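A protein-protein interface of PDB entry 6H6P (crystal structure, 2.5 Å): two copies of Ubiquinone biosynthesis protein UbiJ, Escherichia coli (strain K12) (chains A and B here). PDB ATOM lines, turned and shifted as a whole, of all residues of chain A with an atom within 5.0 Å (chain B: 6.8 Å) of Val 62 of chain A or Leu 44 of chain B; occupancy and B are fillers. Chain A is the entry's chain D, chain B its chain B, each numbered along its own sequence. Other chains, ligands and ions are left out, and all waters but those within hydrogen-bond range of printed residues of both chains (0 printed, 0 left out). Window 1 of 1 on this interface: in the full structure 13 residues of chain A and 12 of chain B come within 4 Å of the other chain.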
ATOM      1  N   LYS A  46     -27.048  -7.681  -8.509  1.00  0.00           N
ATOM      2  CA  LYS A  46     -25.935  -6.754  -8.260  1.00  0.00           C
ATOM      3  C   LYS A  46     -24.606  -7.463  -8.097  1.00  0.00           C
ATOM      4  O   LYS A  46     -24.544  -8.581  -7.620  1.00  0.00           O
ATOM      5  CB  LYS A  46     -26.203  -5.823  -7.063  1.00  0.00           C
ATOM      6  CG  LYS A  46     -27.495  -5.002  -7.132  1.00  0.00           C
ATOM      7  CD  LYS A  46     -27.394  -3.853  -8.086  1.00  0.00           C
ATOM      8  CE  LYS A  46     -28.737  -3.283  -8.421  1.00  0.00           C
ATOM      9  NZ  LYS A  46     -28.636  -2.316  -9.535  1.00  0.00           N
ATOM     10  N   VAL A  47     -23.541  -6.788  -8.518  1.00  0.00           N
ATOM     11  CA  VAL A  47     -22.155  -7.221  -8.446  1.00  0.00           C
ATOM     12  C   VAL A  47     -21.411  -6.164  -7.633  1.00  0.00           C
ATOM     13  O   VAL A  47     -21.442  -4.972  -7.971  1.00  0.00           O
ATOM     14  CB  VAL A  47     -21.526  -7.451  -9.852  1.00  0.00           C
ATOM     15  CG1 VAL A  47     -20.073  -7.920  -9.727  1.00  0.00           C
ATOM     16  CG2 VAL A  47     -22.343  -8.452 -10.658  1.00  0.00           C
ATOM     17  N   ILE A  60     -15.033 -10.508  -5.933  1.00  0.00           N
ATOM     18  CA  ILE A  60     -16.226 -10.043  -6.629  1.00  0.00           C
ATOM     19  C   ILE A  60     -17.429 -10.817  -6.095  1.00  0.00           C
ATOM     20  O   ILE A  60     -17.431 -12.038  -6.184  1.00  0.00           O
ATOM     21  CB  ILE A  60     -16.051 -10.148  -8.175  1.00  0.00           C
ATOM     22  CG1 ILE A  60     -14.760  -9.433  -8.669  1.00  0.00           C
ATOM     23  CG2 ILE A  60     -17.283  -9.614  -8.890  1.00  0.00           C
ATOM     24  CD1 ILE A  60     -13.566 -10.309  -8.917  1.00  0.00           C
ATOM     25  N   LEU A  61     -18.412 -10.122  -5.483  1.00  0.00           N
ATOM     26  CA  LEU A  61     -19.621 -10.744  -4.950  1.00  0.00           C
ATOM     27  C   LEU A  61     -20.759 -10.537  -5.917  1.00  0.00           C
ATOM     28  O   LEU A  61     -21.051  -9.392  -6.251  1.00  0.00           O
ATOM     29  CB  LEU A  61     -20.051 -10.168  -3.573  1.00  0.00           C
ATOM     30  CG  LEU A  61     -19.036  -9.832  -2.478  1.00  0.00           C
ATOM     31  CD1 LEU A  61     -19.759  -9.452  -1.213  1.00  0.00           C
ATOM     32  CD2 LEU A  61     -18.187 -10.996  -2.157  1.00  0.00           C
ATOM     33  N   VAL A  62     -21.404 -11.633  -6.367  1.00  0.00           N
ATOM     34  CA  VAL A  62     -22.568 -11.598  -7.264  1.00  0.00           C
ATOM     35  C   VAL A  62     -23.791 -12.059  -6.457  1.00  0.00           C
ATOM     36  O   VAL A  62     -23.774 -13.159  -5.909  1.00  0.00           O
ATOM     37  CB  VAL A  62     -22.344 -12.424  -8.561  1.00  0.00           C
ATOM     38  CG1 VAL A  62     -23.478 -12.185  -9.553  1.00  0.00           C
ATOM     39  CG2 VAL A  62     -20.988 -12.087  -9.193  1.00  0.00           C
ATOM     40  N   PHE A  63     -24.803 -11.187  -6.305  1.00  0.00           N
ATOM     41  CA  PHE A  63     -25.995 -11.485  -5.502  1.00  0.00           C
ATOM     42  C   PHE A  63     -27.216 -11.958  -6.321  1.00  0.00           C
ATOM     43  O   PHE A  63     -27.696 -11.266  -7.226  1.00  0.00           O
ATOM     44  CB  PHE A  63     -26.375 -10.311  -4.612  1.00  0.00           C
ATOM     45  CG  PHE A  63     -25.247  -9.740  -3.802  1.00  0.00           C
ATOM     46  CD1 PHE A  63     -24.499  -8.666  -4.278  1.00  0.00           C
ATOM     47  CD2 PHE A  63     -24.961 -10.235  -2.537  1.00  0.00           C
ATOM     48  CE1 PHE A  63     -23.465  -8.116  -3.512  1.00  0.00           C
ATOM     49  CE2 PHE A  63     -23.903  -9.704  -1.787  1.00  0.00           C
ATOM     50  CZ  PHE A  63     -23.172  -8.642  -2.274  1.00  0.00           C
ATOM     51  N   SER A  64     -27.711 -13.156  -5.965  1.00  0.00           N
ATOM     52  CA  SER A  64     -28.868 -13.830  -6.543  1.00  0.00           C
ATOM     53  C   SER A  64     -29.992 -13.864  -5.476  1.00  0.00           C
ATOM     54  O   SER A  64     -29.890 -13.219  -4.425  1.00  0.00           O
ATOM     55  CB  SER A  64     -28.488 -15.241  -6.996  1.00  0.00           C
ATOM     56  OG  SER A  64     -27.086 -15.462  -7.021  1.00  0.00           O
ATOM     57  N   GLN A  67     -28.592 -17.236  -3.266  1.00  0.00           N
ATOM     58  CA  GLN A  67     -27.153 -17.314  -2.950  1.00  0.00           C
ATOM     59  C   GLN A  67     -26.347 -16.062  -3.345  1.00  0.00           C
ATOM     60  O   GLN A  67     -26.867 -15.194  -4.046  1.00  0.00           O
ATOM     61  CB  GLN A  67     -26.507 -18.583  -3.554  1.00  0.00           C
ATOM     62  CG  GLN A  67     -26.597 -18.667  -5.064  1.00  0.00           C
ATOM     63  CD  GLN A  67     -25.839 -19.843  -5.635  1.00  0.00           C
ATOM     64  OE1 GLN A  67     -25.745 -20.913  -5.032  1.00  0.00           O
ATOM     65  NE2 GLN A  67     -25.286 -19.677  -6.833  1.00  0.00           N
ATOM     66  N   VAL A  68     -25.089 -15.976  -2.854  1.00  0.00           N
ATOM     67  CA  VAL A  68     -24.062 -14.973  -3.199  1.00  0.00           C
ATOM     68  C   VAL A  68     -22.850 -15.761  -3.707  1.00  0.00           C
ATOM     69  O   VAL A  68     -22.421 -16.699  -3.032  1.00  0.00           O
ATOM     70  CB  VAL A  68     -23.668 -13.920  -2.098  1.00  0.00           C
ATOM     71  CG1 VAL A  68     -23.142 -14.576  -0.829  1.00  0.00           C
ATOM     72  CG2 VAL A  68     -22.648 -12.904  -2.621  1.00  0.00           C
ATOM     73  N   ASP A  69     -22.351 -15.432  -4.909  1.00  0.00           N
ATOM     74  CA  ASP A  69     -21.146 -16.064  -5.504  1.00  0.00           C
ATOM     75  C   ASP A  69     -19.932 -15.164  -5.261  1.00  0.00           C
ATOM     76  O   ASP A  69     -20.045 -13.950  -5.409  1.00  0.00           O
ATOM     77  CB  ASP A  69     -21.327 -16.332  -7.017  1.00  0.00           C
ATOM     78  CG  ASP A  69     -22.589 -17.115  -7.351  1.00  0.00           C
ATOM     79  OD1 ASP A  69     -22.814 -18.191  -6.739  1.00  0.00           O
ATOM     80  OD2 ASP A  69     -23.340 -16.667  -8.225  1.00  0.00           O
ATOM     81  N   LEU A  71     -16.112 -14.561  -6.377  1.00  0.00           N
ATOM     82  CA  LEU A  71     -15.128 -14.812  -7.429  1.00  0.00           C
ATOM     83  C   LEU A  71     -13.834 -14.063  -7.153  1.00  0.00           C
ATOM     84  O   LEU A  71     -13.858 -12.952  -6.627  1.00  0.00           O
ATOM     85  CB  LEU A  71     -15.666 -14.364  -8.807  1.00  0.00           C
ATOM     86  CG  LEU A  71     -17.126 -14.648  -9.150  1.00  0.00           C
ATOM     87  CD1 LEU A  71     -17.562 -13.801 -10.270  1.00  0.00           C
ATOM     88  CD2 LEU A  71     -17.330 -16.054  -9.529  1.00  0.00           C
ATOM     89  N   TRP A  74     -12.819 -11.368 -12.282  1.00  0.00           N
ATOM     90  CA  TRP A  74     -13.916 -11.017 -13.169  1.00  0.00           C
ATOM     91  C   TRP A  74     -13.448  -9.958 -14.133  1.00  0.00           C
ATOM     92  O   TRP A  74     -12.844  -8.958 -13.724  1.00  0.00           O
ATOM     93  CB  TRP A  74     -15.241 -10.640 -12.464  1.00  0.00           C
ATOM     94  CG  TRP A  74     -16.442 -10.793 -13.366  1.00  0.00           C
ATOM     95  CD1 TRP A  74     -16.703 -11.830 -14.218  1.00  0.00           C
ATOM     96  CD2 TRP A  74     -17.534  -9.871 -13.513  1.00  0.00           C
ATOM     97  NE1 TRP A  74     -17.861 -11.588 -14.923  1.00  0.00           N
ATOM     98  CE2 TRP A  74     -18.399 -10.398 -14.501  1.00  0.00           C
ATOM     99  CE3 TRP A  74     -17.879  -8.654 -12.891  1.00  0.00           C
ATOM    100  CZ2 TRP A  74     -19.578  -9.743 -14.891  1.00  0.00           C
ATOM    101  CZ3 TRP A  74     -19.046  -8.011 -13.278  1.00  0.00           C
ATOM    102  CH2 TRP A  74     -19.892  -8.565 -14.249  1.00  0.00           C
ATOM    103  N   TYR B  31     -26.442 -24.836 -16.621  1.00  0.00           N
ATOM    104  CA  TYR B  31     -25.609 -24.675 -15.432  1.00  0.00           C
ATOM    105  C   TYR B  31     -24.978 -25.966 -14.910  1.00  0.00           C
ATOM    106  O   TYR B  31     -24.361 -25.935 -13.842  1.00  0.00           O
ATOM    107  CB  TYR B  31     -26.407 -23.940 -14.328  1.00  0.00           C
ATOM    108  CG  TYR B  31     -26.535 -22.471 -14.651  1.00  0.00           C
ATOM    109  CD1 TYR B  31     -27.467 -22.018 -15.577  1.00  0.00           C
ATOM    110  CD2 TYR B  31     -25.664 -21.543 -14.104  1.00  0.00           C
ATOM    111  CE1 TYR B  31     -27.515 -20.679 -15.964  1.00  0.00           C
ATOM    112  CE2 TYR B  31     -25.731 -20.189 -14.452  1.00  0.00           C
ATOM    113  CZ  TYR B  31     -26.651 -19.764 -15.392  1.00  0.00           C
ATOM    114  OH  TYR B  31     -26.717 -18.446 -15.767  1.00  0.00           O
ATOM    115  N   ALA B  39     -19.374 -18.889 -21.187  1.00  0.00           N
ATOM    116  CA  ALA B  39     -20.648 -18.376 -21.717  1.00  0.00           C
ATOM    117  C   ALA B  39     -21.541 -17.851 -20.589  1.00  0.00           C
ATOM    118  O   ALA B  39     -22.188 -16.817 -20.757  1.00  0.00           O
ATOM    119  CB  ALA B  39     -21.373 -19.466 -22.493  1.00  0.00           C
ATOM    120  N   ARG B  40     -21.533 -18.555 -19.422  1.00  0.00           N
ATOM    121  CA  ARG B  40     -22.293 -18.251 -18.194  1.00  0.00           C
ATOM    122  C   ARG B  40     -21.806 -16.963 -17.526  1.00  0.00           C
ATOM    123  O   ARG B  40     -22.623 -16.225 -16.962  1.00  0.00           O
ATOM    124  CB  ARG B  40     -22.174 -19.420 -17.178  1.00  0.00           C
ATOM    125  CG  ARG B  40     -23.057 -20.642 -17.470  1.00  0.00           C
ATOM    126  CD  ARG B  40     -23.166 -21.579 -16.314  1.00  0.00           C
ATOM    127  NE  ARG B  40     -21.910 -22.222 -15.921  1.00  0.00           N
ATOM    128  CZ  ARG B  40     -21.600 -23.485 -16.183  1.00  0.00           C
ATOM    129  NH1 ARG B  40     -22.417 -24.241 -16.891  1.00  0.00           N
ATOM    130  NH2 ARG B  40     -20.457 -23.994 -15.761  1.00  0.00           N
ATOM    131  N   SER B  41     -20.469 -16.744 -17.545  1.00  0.00           N
ATOM    132  CA  SER B  41     -19.744 -15.618 -16.937  1.00  0.00           C
ATOM    133  C   SER B  41     -19.972 -14.265 -17.615  1.00  0.00           C
ATOM    134  O   SER B  41     -19.727 -13.224 -17.008  1.00  0.00           O
ATOM    135  CB  SER B  41     -18.256 -15.928 -16.848  1.00  0.00           C
ATOM    136  OG  SER B  41     -17.650 -16.014 -18.128  1.00  0.00           O
ATOM    137  N   ARG B  42     -20.438 -14.284 -18.870  1.00  0.00           N
ATOM    138  CA  ARG B  42     -20.783 -13.115 -19.678  1.00  0.00           C
ATOM    139  C   ARG B  42     -22.161 -12.577 -19.238  1.00  0.00           C
ATOM    140  O   ARG B  42     -22.509 -11.424 -19.542  1.00  0.00           O
ATOM    141  CB  ARG B  42     -20.853 -13.512 -21.148  1.00  0.00           C
ATOM    142  CG  ARG B  42     -19.503 -13.888 -21.704  1.00  0.00           C
ATOM    143  CD  ARG B  42     -19.423 -13.776 -23.206  1.00  0.00           C
ATOM    144  NE  ARG B  42     -18.021 -13.883 -23.592  1.00  0.00           N
ATOM    145  CZ  ARG B  42     -17.414 -15.017 -23.938  1.00  0.00           C
ATOM    146  NH1 ARG B  42     -16.123 -15.020 -24.238  1.00  0.00           N
ATOM    147  NH2 ARG B  42     -18.097 -16.154 -23.999  1.00  0.00           N
ATOM    148  N   LEU B  43     -22.945 -13.438 -18.541  1.00  0.00           N
ATOM    149  CA  LEU B  43     -24.285 -13.157 -18.036  1.00  0.00           C
ATOM    150  C   LEU B  43     -24.340 -12.804 -16.562  1.00  0.00           C
ATOM    151  O   LEU B  43     -25.384 -12.410 -16.079  1.00  0.00           O
ATOM    152  CB  LEU B  43     -25.233 -14.321 -18.343  1.00  0.00           C
ATOM    153  CG  LEU B  43     -25.651 -14.513 -19.796  1.00  0.00           C
ATOM    154  CD1 LEU B  43     -26.234 -15.898 -19.988  1.00  0.00           C
ATOM    155  CD2 LEU B  43     -26.617 -13.386 -20.246  1.00  0.00           C
ATOM    156  N   LEU B  44     -23.212 -12.890 -15.866  1.00  0.00           N
ATOM    157  CA  LEU B  44     -23.029 -12.565 -14.455  1.00  0.00           C
ATOM    158  C   LEU B  44     -23.565 -11.189 -14.028  1.00  0.00           C
ATOM    159  O   LEU B  44     -23.041 -10.140 -14.427  1.00  0.00           O
ATOM    160  CB  LEU B  44     -21.552 -12.703 -14.075  1.00  0.00           C
ATOM    161  CG  LEU B  44     -21.123 -14.024 -13.475  1.00  0.00           C
ATOM    162  CD1 LEU B  44     -19.633 -14.053 -13.274  1.00  0.00           C
ATOM    163  CD2 LEU B  44     -21.764 -14.236 -12.144  1.00  0.00           C
ATOM    164  N   GLY B  45     -24.605 -11.247 -13.192  1.00  0.00           N
ATOM    165  CA  GLY B  45     -25.289 -10.098 -12.613  1.00  0.00           C
ATOM    166  C   GLY B  45     -26.301  -9.458 -13.542  1.00  0.00           C
ATOM    167  O   GLY B  45     -26.771  -8.349 -13.268  1.00  0.00           O
ATOM    168  N   LYS B  46     -26.640 -10.139 -14.657  1.00  0.00           N
ATOM    169  CA  LYS B  46     -27.605  -9.635 -15.639  1.00  0.00           C
ATOM    170  C   LYS B  46     -29.008 -10.156 -15.388  1.00  0.00           C
ATOM    171  O   LYS B  46     -29.190 -11.301 -14.983  1.00  0.00           O
ATOM    172  CB  LYS B  46     -27.191  -9.967 -17.088  1.00  0.00           C
ATOM    173  CG  LYS B  46     -25.847  -9.417 -17.519  1.00  0.00           C
ATOM    174  CD  LYS B  46     -25.893  -7.917 -17.740  1.00  0.00           C
ATOM    175  CE  LYS B  46     -24.522  -7.324 -17.741  1.00  0.00           C
ATOM    176  NZ  LYS B  46     -24.605  -5.848 -17.661  1.00  0.00           N
ATOM    177  N   PHE B  63     -29.064 -13.963 -13.739  1.00  0.00           N
ATOM    178  CA  PHE B  63     -27.920 -14.845 -13.961  1.00  0.00           C
ATOM    179  C   PHE B  63     -26.784 -14.655 -12.970  1.00  0.00           C
ATOM    180  O   PHE B  63     -26.251 -13.559 -12.865  1.00  0.00           O
ATOM    181  CB  PHE B  63     -27.412 -14.732 -15.411  1.00  0.00           C
ATOM    182  CG  PHE B  63     -28.463 -14.992 -16.471  1.00  0.00           C
ATOM    183  CD1 PHE B  63     -28.679 -16.272 -16.962  1.00  0.00           C
ATOM    184  CD2 PHE B  63     -29.212 -13.952 -16.997  1.00  0.00           C
ATOM    185  CE1 PHE B  63     -29.623 -16.503 -17.955  1.00  0.00           C
ATOM    186  CE2 PHE B  63     -30.143 -14.182 -17.995  1.00  0.00           C
ATOM    187  CZ  PHE B  63     -30.368 -15.457 -18.441  1.00  0.00           C
ATOM    188  N   SER B  64     -26.406 -15.755 -12.269  1.00  0.00           N
ATOM    189  CA  SER B  64     -25.342 -15.855 -11.273  1.00  0.00           C
ATOM    190  C   SER B  64     -24.236 -16.772 -11.821  1.00  0.00           C
ATOM    191  O   SER B  64     -24.281 -17.139 -12.993  1.00  0.00           O
ATOM    192  CB  SER B  64     -25.887 -16.383  -9.947  1.00  0.00           C
ATOM    193  OG  SER B  64     -27.305 -16.365  -9.888  1.00  0.00           O
ATOM    194  N   GLU B  65     -23.222 -17.103 -10.999  1.00  0.00           N
ATOM    195  CA  GLU B  65     -22.103 -17.963 -11.398  1.00  0.00           C
ATOM    196  C   GLU B  65     -22.541 -19.438 -11.435  1.00  0.00           C
ATOM    197  O   GLU B  65     -22.174 -20.168 -12.352  1.00  0.00           O
ATOM    198  CB  GLU B  65     -20.896 -17.754 -10.449  1.00  0.00           C
ATOM    199  CG  GLU B  65     -19.720 -18.705 -10.648  1.00  0.00           C
ATOM    200  CD  GLU B  65     -18.745 -18.909  -9.497  1.00  0.00           C
ATOM    201  OE1 GLU B  65     -17.559 -19.192  -9.785  1.00  0.00           O
ATOM    202  OE2 GLU B  65     -19.157 -18.808  -8.317  1.00  0.00           O
ATOM    203  N   ARG B  66     -23.324 -19.862 -10.441  1.00  0.00           N
ATOM    204  CA  ARG B  66     -23.732 -21.248 -10.244  1.00  0.00           C
ATOM    205  C   ARG B  66     -25.189 -21.553 -10.579  1.00  0.00           C
ATOM    206  O   ARG B  66     -25.560 -22.730 -10.580  1.00  0.00           O
ATOM    207  CB  ARG B  66     -23.421 -21.688  -8.786  1.00  0.00           C
ATOM    208  CG  ARG B  66     -21.946 -21.759  -8.386  1.00  0.00           C
ATOM    209  CD  ARG B  66     -21.678 -21.209  -6.970  1.00  0.00           C
ATOM    210  NE  ARG B  66     -22.252 -21.999  -5.882  1.00  0.00           N
ATOM    211  CZ  ARG B  66     -22.395 -21.561  -4.631  1.00  0.00           C
ATOM    212  NH1 ARG B  66     -22.067 -20.313  -4.313  1.00  0.00           N
ATOM    213  NH2 ARG B  66     -22.905 -22.354  -3.700  1.00  0.00           N
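Gly 45 of chain B touches Val 47 of chain A. CG1 of Val 62 of chain A touches CD2 of Leu 44 of chain B (3.7 Å). CG1 of Val 62 of chain A touches N of Gly 45 of chain B, 3.9 Å away. NH1 of Arg 66 of chain B touches O of Val 68 of chain A (3.9 Å). OD2 of Asp 69 of chain A touches CB of Ser 64 of chain B, 3.1 Å away. Leu 44 of chain B touches Leu 71 of chain A (CD1 to CD1, 3.7 Å). Glu 65 of chain B touches Leu 71 of chain A. Leu 44 of chain B touches Trp 74 of chain A.
N of Gly 45 of chain B is in hydrogen-bond range of O of Phe 63 of chain B (2.9 Å). N of Ile 60 of chain A is in hydrogen-bond range of O of Leu 71 of chain A, 2.8 Å away. The backbone NH (N) of Val 62 of chain A sits at hydrogen-bond distance from the backbone carbonyl oxygen (O) of Asp 69 of chain A, 2.9 Å away. The backbone carbonyl oxygen of Gln 67 of chain A lies within hydrogen-bond range of the side-chain hydroxyl of Ser 64 of chain A (3.0 Å). The side-chain amide nitrogen of Gln 67 of chain A is in hydrogen-bond range of the side-chain carboxylate of Asp 69 of chain A, at 2.9 Å.
Printed residues of chain B that touch a printed residue of chain A: Ser 41, Leu 44, Gly 45, Ser 64, Glu 65 and Arg 66. Hydrophobic or aromatic side chains of chain B within 4 Å of the printed part of chain A: Leu 44. Hydrophobic or aromatic side chains of chain A that line the printed part of chain B: Val 47, Val 62, Leu 71 and Trp 74. Among the printed residues, Asp or Glu carboxylates within 4 Å of a Lys or Arg side-chain nitrogen of the other chain: Asp 69 of chain A with Arg 66 of chain B (3.3 Å).
Val 62 of chain A touches just these residues of chain B: Leu 44 and Gly 45. Of the printed residues of chain B, Val 68 of chain A touches Arg 66 (3.9 Å). Of the printed residues of chain A, Ser 41 of chain B touches Trp 74. Printed residues of chain A within 4 Å of Gly 45 of chain B: Val 47 and Val 62. Printed residues of chain A within 4 Å of Ser 64 of chain B: Ser 64 (3.0 Å) and Asp 69 (3.1 Å). The nearest residue of chain B that does not touch Val 62 of chain A is Ser 64 of chain B (4.5 Å). The nearest residue of chain A that does not touch Leu 44 of chain B is Val 47 of chain A (4.2 Å).
Ser 64 of chain B touches its own counterpart, Ser 64 of chain A. 3 positions are printed for both chains.
The backbone carbonyl oxygen (O) of Ser 41 of chain B sits at hydrogen-bond distance from the indole nitrogen (NE1) of Trp 74 of chain A, 3.2 Å away. The side-chain hydroxyl of Ser 64 of chain B lies within hydrogen-bond range of the side-chain hydroxyl of Ser 64 of chain A, at 3.0 Å. N of Glu 65 of chain B is in hydrogen-bond range of OD2 of Asp 69 of chain A. The side-chain amide oxygen of Gln 67 of chain A sits close to the guanidinium group of Arg 66 of chain B, at 3.5 Å. The side-chain carboxylate (OD1) of Asp 69 of chain A lies within salt-bridge range of the guanidinium group (NH1) of Arg 66 of chain B (3.3 Å).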
